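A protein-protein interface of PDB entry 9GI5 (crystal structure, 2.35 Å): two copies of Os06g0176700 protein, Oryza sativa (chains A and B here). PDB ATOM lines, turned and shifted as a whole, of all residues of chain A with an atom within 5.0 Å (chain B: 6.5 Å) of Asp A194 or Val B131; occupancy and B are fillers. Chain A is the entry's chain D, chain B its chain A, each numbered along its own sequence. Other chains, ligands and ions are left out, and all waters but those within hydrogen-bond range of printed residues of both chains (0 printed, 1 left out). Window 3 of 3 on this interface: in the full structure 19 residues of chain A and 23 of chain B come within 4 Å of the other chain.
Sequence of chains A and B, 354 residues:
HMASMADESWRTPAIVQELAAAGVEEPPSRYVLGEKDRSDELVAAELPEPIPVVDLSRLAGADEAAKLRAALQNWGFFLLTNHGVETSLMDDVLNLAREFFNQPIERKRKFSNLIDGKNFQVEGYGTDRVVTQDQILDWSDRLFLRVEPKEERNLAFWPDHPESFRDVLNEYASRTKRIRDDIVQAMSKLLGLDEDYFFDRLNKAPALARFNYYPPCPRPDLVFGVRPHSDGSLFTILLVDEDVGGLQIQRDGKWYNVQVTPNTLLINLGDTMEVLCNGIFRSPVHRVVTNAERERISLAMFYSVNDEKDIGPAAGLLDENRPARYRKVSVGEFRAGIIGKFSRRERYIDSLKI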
ATOM      1  N   SER A 188      20.128 -16.528  24.147  1.00  0.00           N
ATOM      2  CA  SER A 188      21.543 -16.229  23.976  1.00  0.00           C
ATOM      3  C   SER A 188      22.316 -16.516  25.254  1.00  0.00           C
ATOM      4  O   SER A 188      23.419 -17.076  25.209  1.00  0.00           O
ATOM      5  CB  SER A 188      21.724 -14.772  23.547  1.00  0.00           C
ATOM      6  OG  SER A 188      21.183 -14.553  22.254  1.00  0.00           O
ATOM      7  N   GLY A 192      25.165 -19.567  26.002  1.00  0.00           N
ATOM      8  CA  GLY A 192      26.515 -19.143  26.306  1.00  0.00           C
ATOM      9  C   GLY A 192      27.094 -18.133  25.344  1.00  0.00           C
ATOM     10  O   GLY A 192      28.318 -18.005  25.261  1.00  0.00           O
ATOM     11  N   LEU A 193      26.253 -17.412  24.612  1.00  0.00           N
ATOM     12  CA  LEU A 193      26.693 -16.363  23.705  1.00  0.00           C
ATOM     13  C   LEU A 193      26.491 -14.993  24.340  1.00  0.00           C
ATOM     14  O   LEU A 193      25.882 -14.851  25.402  1.00  0.00           O
ATOM     15  CB  LEU A 193      25.928 -16.438  22.378  1.00  0.00           C
ATOM     16  CG  LEU A 193      25.785 -17.814  21.730  1.00  0.00           C
ATOM     17  CD1 LEU A 193      24.637 -17.806  20.738  1.00  0.00           C
ATOM     18  CD2 LEU A 193      27.081 -18.210  21.052  1.00  0.00           C
ATOM     19  N   ASP A 194      27.018 -13.973  23.668  1.00  0.00           N
ATOM     20  CA  ASP A 194      26.669 -12.604  24.015  1.00  0.00           C
ATOM     21  C   ASP A 194      25.160 -12.434  23.938  1.00  0.00           C
ATOM     22  O   ASP A 194      24.518 -12.916  23.002  1.00  0.00           O
ATOM     23  CB  ASP A 194      27.358 -11.630  23.063  1.00  0.00           C
ATOM     24  CG  ASP A 194      28.856 -11.604  23.248  1.00  0.00           C
ATOM     25  OD1 ASP A 194      29.321 -11.145  24.318  1.00  0.00           O
ATOM     26  OD2 ASP A 194      29.568 -12.055  22.328  1.00  0.00           O
ATOM     27  N   GLU A 195      24.576 -11.761  24.931  1.00  0.00           N
ATOM     28  CA  GLU A 195      23.120 -11.671  24.895  1.00  0.00           C
ATOM     29  C   GLU A 195      22.606 -10.737  23.809  1.00  0.00           C
ATOM     30  O   GLU A 195      21.394 -10.707  23.578  1.00  0.00           O
ATOM     31  CB  GLU A 195      22.531 -11.264  26.251  1.00  0.00           C
ATOM     32  CG  GLU A 195      23.232 -10.171  27.032  1.00  0.00           C
ATOM     33  CD  GLU A 195      22.881 -10.255  28.516  1.00  0.00           C
ATOM     34  OE1 GLU A 195      21.701 -10.005  28.855  1.00  0.00           O
ATOM     35  OE2 GLU A 195      23.759 -10.631  29.328  1.00  0.00           O
ATOM     36  N   ASP A 196      23.475  -9.991  23.136  1.00  0.00           N
ATOM     37  CA  ASP A 196      23.084  -9.235  21.953  1.00  0.00           C
ATOM     38  C   ASP A 196      23.507  -9.919  20.657  1.00  0.00           C
ATOM     39  O   ASP A 196      23.453  -9.291  19.595  1.00  0.00           O
ATOM     40  CB  ASP A 196      23.653  -7.812  22.007  1.00  0.00           C
ATOM     41  CG  ASP A 196      25.167  -7.788  22.145  1.00  0.00           C
ATOM     42  OD1 ASP A 196      25.752  -8.767  22.660  1.00  0.00           O
ATOM     43  OD2 ASP A 196      25.773  -6.772  21.744  1.00  0.00           O
ATOM     44  N   TYR A 197      23.896 -11.199  20.721  1.00  0.00           N
ATOM     45  CA  TYR A 197      24.480 -11.872  19.560  1.00  0.00           C
ATOM     46  C   TYR A 197      23.533 -11.879  18.368  1.00  0.00           C
ATOM     47  O   TYR A 197      23.971 -11.739  17.221  1.00  0.00           O
ATOM     48  CB  TYR A 197      24.884 -13.307  19.923  1.00  0.00           C
ATOM     49  CG  TYR A 197      25.317 -14.161  18.744  1.00  0.00           C
ATOM     50  CD1 TYR A 197      24.390 -14.855  17.966  1.00  0.00           C
ATOM     51  CD2 TYR A 197      26.657 -14.255  18.398  1.00  0.00           C
ATOM     52  CE1 TYR A 197      24.794 -15.624  16.883  1.00  0.00           C
ATOM     53  CE2 TYR A 197      27.069 -15.019  17.320  1.00  0.00           C
ATOM     54  CZ  TYR A 197      26.135 -15.701  16.567  1.00  0.00           C
ATOM     55  OH  TYR A 197      26.557 -16.457  15.494  1.00  0.00           O
ATOM     56  N   TRP B  10      35.051 -20.691  36.075  1.00  0.00           N
ATOM     57  CA  TRP B  10      35.111 -19.268  35.766  1.00  0.00           C
ATOM     58  C   TRP B  10      33.729 -18.663  35.544  1.00  0.00           C
ATOM     59  O   TRP B  10      33.580 -17.440  35.642  1.00  0.00           O
ATOM     60  CB  TRP B  10      36.001 -19.019  34.544  1.00  0.00           C
ATOM     61  CG  TRP B  10      35.613 -19.767  33.299  1.00  0.00           C
ATOM     62  CD1 TRP B  10      36.103 -20.968  32.881  1.00  0.00           C
ATOM     63  CD2 TRP B  10      34.674 -19.347  32.299  1.00  0.00           C
ATOM     64  NE1 TRP B  10      35.520 -21.330  31.692  1.00  0.00           N
ATOM     65  CE2 TRP B  10      34.639 -20.353  31.313  1.00  0.00           C
ATOM     66  CE3 TRP B  10      33.854 -18.221  32.145  1.00  0.00           C
ATOM     67  CZ2 TRP B  10      33.817 -20.269  30.187  1.00  0.00           C
ATOM     68  CZ3 TRP B  10      33.037 -18.140  31.029  1.00  0.00           C
ATOM     69  CH2 TRP B  10      33.026 -19.158  30.065  1.00  0.00           C
ATOM     70  N   ARG B  11      32.716 -19.481  35.259  1.00  0.00           N
ATOM     71  CA  ARG B  11      31.348 -18.980  35.222  1.00  0.00           C
ATOM     72  C   ARG B  11      30.775 -18.724  36.609  1.00  0.00           C
ATOM     73  O   ARG B  11      29.692 -18.135  36.704  1.00  0.00           O
ATOM     74  CB  ARG B  11      30.435 -19.957  34.476  1.00  0.00           C
ATOM     75  CG  ARG B  11      30.913 -20.318  33.090  1.00  0.00           C
ATOM     76  CD  ARG B  11      29.871 -21.130  32.360  1.00  0.00           C
ATOM     77  NE  ARG B  11      30.344 -21.539  31.044  1.00  0.00           N
ATOM     78  CZ  ARG B  11      30.054 -20.899  29.921  1.00  0.00           C
ATOM     79  NH1 ARG B  11      29.286 -19.823  29.922  1.00  0.00           N
ATOM     80  NH2 ARG B  11      30.549 -21.345  28.770  1.00  0.00           N
ATOM     81  N   ASP B 128      28.447  -9.054  37.605  1.00  0.00           N
ATOM     82  CA  ASP B 128      27.783  -9.101  36.316  1.00  0.00           C
ATOM     83  C   ASP B 128      28.246 -10.316  35.513  1.00  0.00           C
ATOM     84  O   ASP B 128      29.227 -10.984  35.851  1.00  0.00           O
ATOM     85  CB  ASP B 128      28.032  -7.798  35.563  1.00  0.00           C
ATOM     86  CG  ASP B 128      27.754  -6.582  36.433  1.00  0.00           C
ATOM     87  OD1 ASP B 128      26.561  -6.336  36.731  1.00  0.00           O
ATOM     88  OD2 ASP B 128      28.726  -5.894  36.831  1.00  0.00           O
ATOM     89  N   ARG B 129      27.521 -10.590  34.430  1.00  0.00           N
ATOM     90  CA  ARG B 129      27.666 -11.856  33.724  1.00  0.00           C
ATOM     91  C   ARG B 129      29.099 -12.062  33.245  1.00  0.00           C
ATOM     92  O   ARG B 129      29.746 -11.142  32.739  1.00  0.00           O
ATOM     93  CB  ARG B 129      26.699 -11.905  32.538  1.00  0.00           C
ATOM     94  CG  ARG B 129      26.792 -13.186  31.717  1.00  0.00           C
ATOM     95  CD  ARG B 129      25.608 -13.337  30.767  1.00  0.00           C
ATOM     96  NE  ARG B 129      25.785 -14.502  29.908  1.00  0.00           N
ATOM     97  CZ  ARG B 129      25.776 -14.481  28.584  1.00  0.00           C
ATOM     98  NH1 ARG B 129      25.540 -13.369  27.910  1.00  0.00           N
ATOM     99  NH2 ARG B 129      26.007 -15.610  27.920  1.00  0.00           N
ATOM    100  N   VAL B 130      29.600 -13.283  33.424  1.00  0.00           N
ATOM    101  CA  VAL B 130      30.917 -13.685  32.940  1.00  0.00           C
ATOM    102  C   VAL B 130      30.678 -14.520  31.689  1.00  0.00           C
ATOM    103  O   VAL B 130      30.304 -15.696  31.774  1.00  0.00           O
ATOM    104  CB  VAL B 130      31.705 -14.457  34.002  1.00  0.00           C
ATOM    105  CG1 VAL B 130      33.134 -14.702  33.531  1.00  0.00           C
ATOM    106  CG2 VAL B 130      31.695 -13.695  35.314  1.00  0.00           C
ATOM    107  N   VAL B 131      30.898 -13.911  30.524  1.00  0.00           N
ATOM    108  CA  VAL B 131      30.560 -14.531  29.245  1.00  0.00           C
ATOM    109  C   VAL B 131      31.692 -15.418  28.740  1.00  0.00           C
ATOM    110  O   VAL B 131      31.447 -16.504  28.204  1.00  0.00           O
ATOM    111  CB  VAL B 131      30.188 -13.439  28.221  1.00  0.00           C
ATOM    112  CG1 VAL B 131      29.887 -14.048  26.852  1.00  0.00           C
ATOM    113  CG2 VAL B 131      29.001 -12.603  28.717  1.00  0.00           C
ATOM    114  N   THR B 132      32.940 -14.982  28.899  1.00  0.00           N
ATOM    115  CA  THR B 132      34.094 -15.724  28.413  1.00  0.00           C
ATOM    116  C   THR B 132      35.106 -15.902  29.534  1.00  0.00           C
ATOM    117  O   THR B 132      35.109 -15.167  30.522  1.00  0.00           O
ATOM    118  CB  THR B 132      34.770 -15.024  27.224  1.00  0.00           C
ATOM    119  OG1 THR B 132      35.333 -13.781  27.662  1.00  0.00           O
ATOM    120  CG2 THR B 132      33.768 -14.761  26.093  1.00  0.00           C
ATOM    121  N   GLN B 133      35.981 -16.893  29.355  1.00  0.00           N
ATOM    122  CA  GLN B 133      37.000 -17.198  30.355  1.00  0.00           C
ATOM    123  C   GLN B 133      38.033 -16.080  30.483  1.00  0.00           C
ATOM    124  O   GLN B 133      38.554 -15.843  31.580  1.00  0.00           O
ATOM    125  CB  GLN B 133      37.682 -18.517  29.997  1.00  0.00           C
ATOM    126  CG  GLN B 133      38.897 -18.860  30.830  1.00  0.00           C
ATOM    127  CD  GLN B 133      39.340 -20.293  30.624  1.00  0.00           C
ATOM    128  OE1 GLN B 133      38.642 -21.082  29.983  1.00  0.00           O
ATOM    129  NE2 GLN B 133      40.503 -20.640  31.161  1.00  0.00           N
ATOM    130  N   GLN B 135      37.521 -12.888  30.062  1.00  0.00           N
ATOM    131  CA  GLN B 135      36.901 -11.607  30.363  1.00  0.00           C
ATOM    132  C   GLN B 135      37.531 -11.003  31.614  1.00  0.00           C
ATOM    133  O   GLN B 135      37.665 -11.673  32.642  1.00  0.00           O
ATOM    134  CB  GLN B 135      35.395 -11.794  30.550  1.00  0.00           C
ATOM    135  CG  GLN B 135      34.644 -10.543  30.944  1.00  0.00           C
ATOM    136  CD  GLN B 135      33.142 -10.767  30.997  1.00  0.00           C
ATOM    137  OE1 GLN B 135      32.566 -11.384  30.102  1.00  0.00           O
ATOM    138  NE2 GLN B 135      32.500 -10.265  32.051  1.00  0.00           N
ATOM    139  N   ALA B 336      19.728  -5.366  25.715  1.00  0.00           N
ATOM    140  CA  ALA B 336      20.678  -6.463  25.553  1.00  0.00           C
ATOM    141  C   ALA B 336      22.012  -5.966  25.012  1.00  0.00           C
ATOM    142  O   ALA B 336      23.067  -6.531  25.342  1.00  0.00           O
ATOM    143  CB  ALA B 336      20.097  -7.535  24.633  1.00  0.00           C
ATOM    144  N   GLY B 340      25.323  -6.559  26.971  1.00  0.00           N
ATOM    145  CA  GLY B 340      26.348  -7.329  26.285  1.00  0.00           C
ATOM    146  C   GLY B 340      27.614  -6.525  26.052  1.00  0.00           C
ATOM    147  O   GLY B 340      28.718  -6.993  26.340  1.00  0.00           O
ATOM    148  N   LYS B 341      27.466  -5.290  25.549  1.00  0.00           N
ATOM    149  CA  LYS B 341      28.633  -4.460  25.259  1.00  0.00           C
ATOM    150  C   LYS B 341      29.392  -4.103  26.533  1.00  0.00           C
ATOM    151  O   LYS B 341      30.618  -3.926  26.500  1.00  0.00           O
ATOM    152  CB  LYS B 341      28.215  -3.187  24.515  1.00  0.00           C
ATOM    153  CG  LYS B 341      27.703  -3.415  23.084  1.00  0.00           C
ATOM    154  CD  LYS B 341      28.748  -3.057  22.044  1.00  0.00           C
ATOM    155  CE  LYS B 341      28.193  -3.182  20.632  1.00  0.00           C
ATOM    156  NZ  LYS B 341      29.256  -3.052  19.591  1.00  0.00           N
ATOM    157  N   SER B 343      29.928  -6.114  29.032  1.00  0.00           N
ATOM    158  CA  SER B 343      30.790  -7.266  29.290  1.00  0.00           C
ATOM    159  C   SER B 343      32.055  -7.249  28.439  1.00  0.00           C
ATOM    160  O   SER B 343      33.089  -7.784  28.859  1.00  0.00           O
ATOM    161  CB  SER B 343      30.028  -8.567  29.026  1.00  0.00           C
ATOM    162  OG  SER B 343      28.887  -8.686  29.857  1.00  0.00           O
ATOM    163  N   ARG B 344      31.991  -6.673  27.240  1.00  0.00           N
ATOM    164  CA  ARG B 344      33.098  -6.694  26.295  1.00  0.00           C
ATOM    165  C   ARG B 344      33.918  -5.407  26.309  1.00  0.00           C
ATOM    166  O   ARG B 344      34.775  -5.224  25.439  1.00  0.00           O
ATOM    167  CB  ARG B 344      32.574  -6.963  24.879  1.00  0.00           C
ATOM    168  CG  ARG B 344      31.674  -8.190  24.749  1.00  0.00           C
ATOM    169  CD  ARG B 344      31.401  -8.550  23.281  1.00  0.00           C
ATOM    170  NE  ARG B 344      30.600  -7.553  22.568  1.00  0.00           N
ATOM    171  CZ  ARG B 344      29.281  -7.426  22.663  1.00  0.00           C
ATOM    172  NH1 ARG B 344      28.569  -8.168  23.498  1.00  0.00           N
ATOM    173  NH2 ARG B 344      28.656  -6.535  21.896  1.00  0.00           N
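The guanidinium group (NH2) of Arg B129 is in hydrogen-bond range of the backbone carbonyl oxygen (O) of Leu A193, 2.6 Å away.
NH1 of Arg B129 lies within salt-bridge range of OE2 of Glu A195 (3.6 Å).
NH1 of Arg B344 lies within salt-bridge range of OD1 of Asp A194.
OD2 of Asp A196 is in salt-bridge range of NH2 of Arg B344 (2.9 Å).
The side-chain amide nitrogen (NE2) of Gln B135 sits at hydrogen-bond distance from the backbone carbonyl oxygen (O) of Arg B129, at 3.0 Å.
The side-chain amide oxygen (OE1) of Gln B135 is in hydrogen-bond range of the backbone NH (N) of Val B131, at 3.1 Å.
The guanidinium group (NH1) of Arg B344 lies within hydrogen-bond range of the backbone carbonyl oxygen (O) of Gly B340 (3.1 Å).
O of Ser A188 is in hydrogen-bond range of N of Leu A193, at 2.9 Å.
C of Gly A192 touches NH2 of Arg B129 (3.8 Å).
Val B131 touches Asp A194 (CG1 to OD1, 3.9 Å).
Glu A195 touches Ala B336 (O to CB, 3.6 Å).
CB of Asp A196 touches O of Ala B336, 3.6 Å away.
Asp A196 touches Gly B340 (OD1 to CA, 3.9 Å).
Of the printed residues of chain B, Asp A194 touches Val B131 (3.9 Å) and Arg B344 (3.2 Å).
Printed residues of chain B within 4 Å of Glu A195: Arg B129 and Ala B336.
Of the printed residues of chain B, Asp A196 touches Ala B336, Gly B340 and Arg B344.
Arg B11 touches none of the printed residues of chain A.
Of chain A, only Asp A194 comes within 4 Å of Val B131.
Gln B135 touches none of the printed residues of chain A.
The nearest residue of chain B that does not touch Asp A194 is Arg B129 (4.1 Å).
The nearest residue of chain A that does not touch Val B131 is Leu A193 (4.3 Å).
Of the 14 printed residues of chain B, 5 touch a printed residue of chain A.
Hydrophobic or aromatic side chains of chain B within 4 Å of the printed part of chain A: Val B131 and Ala B336.
Among the printed residues, Asp or Glu carboxylates within 4 Å of a Lys or Arg side-chain nitrogen of the other chain: Asp A194 with Arg B344, Glu A195 with Arg B129 and Asp A196 with Arg B344.
No position is printed for both chains.
Of the 9 pairs that touch across the chains among the printed residues, none has its exchanged pair printed and touching as well.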
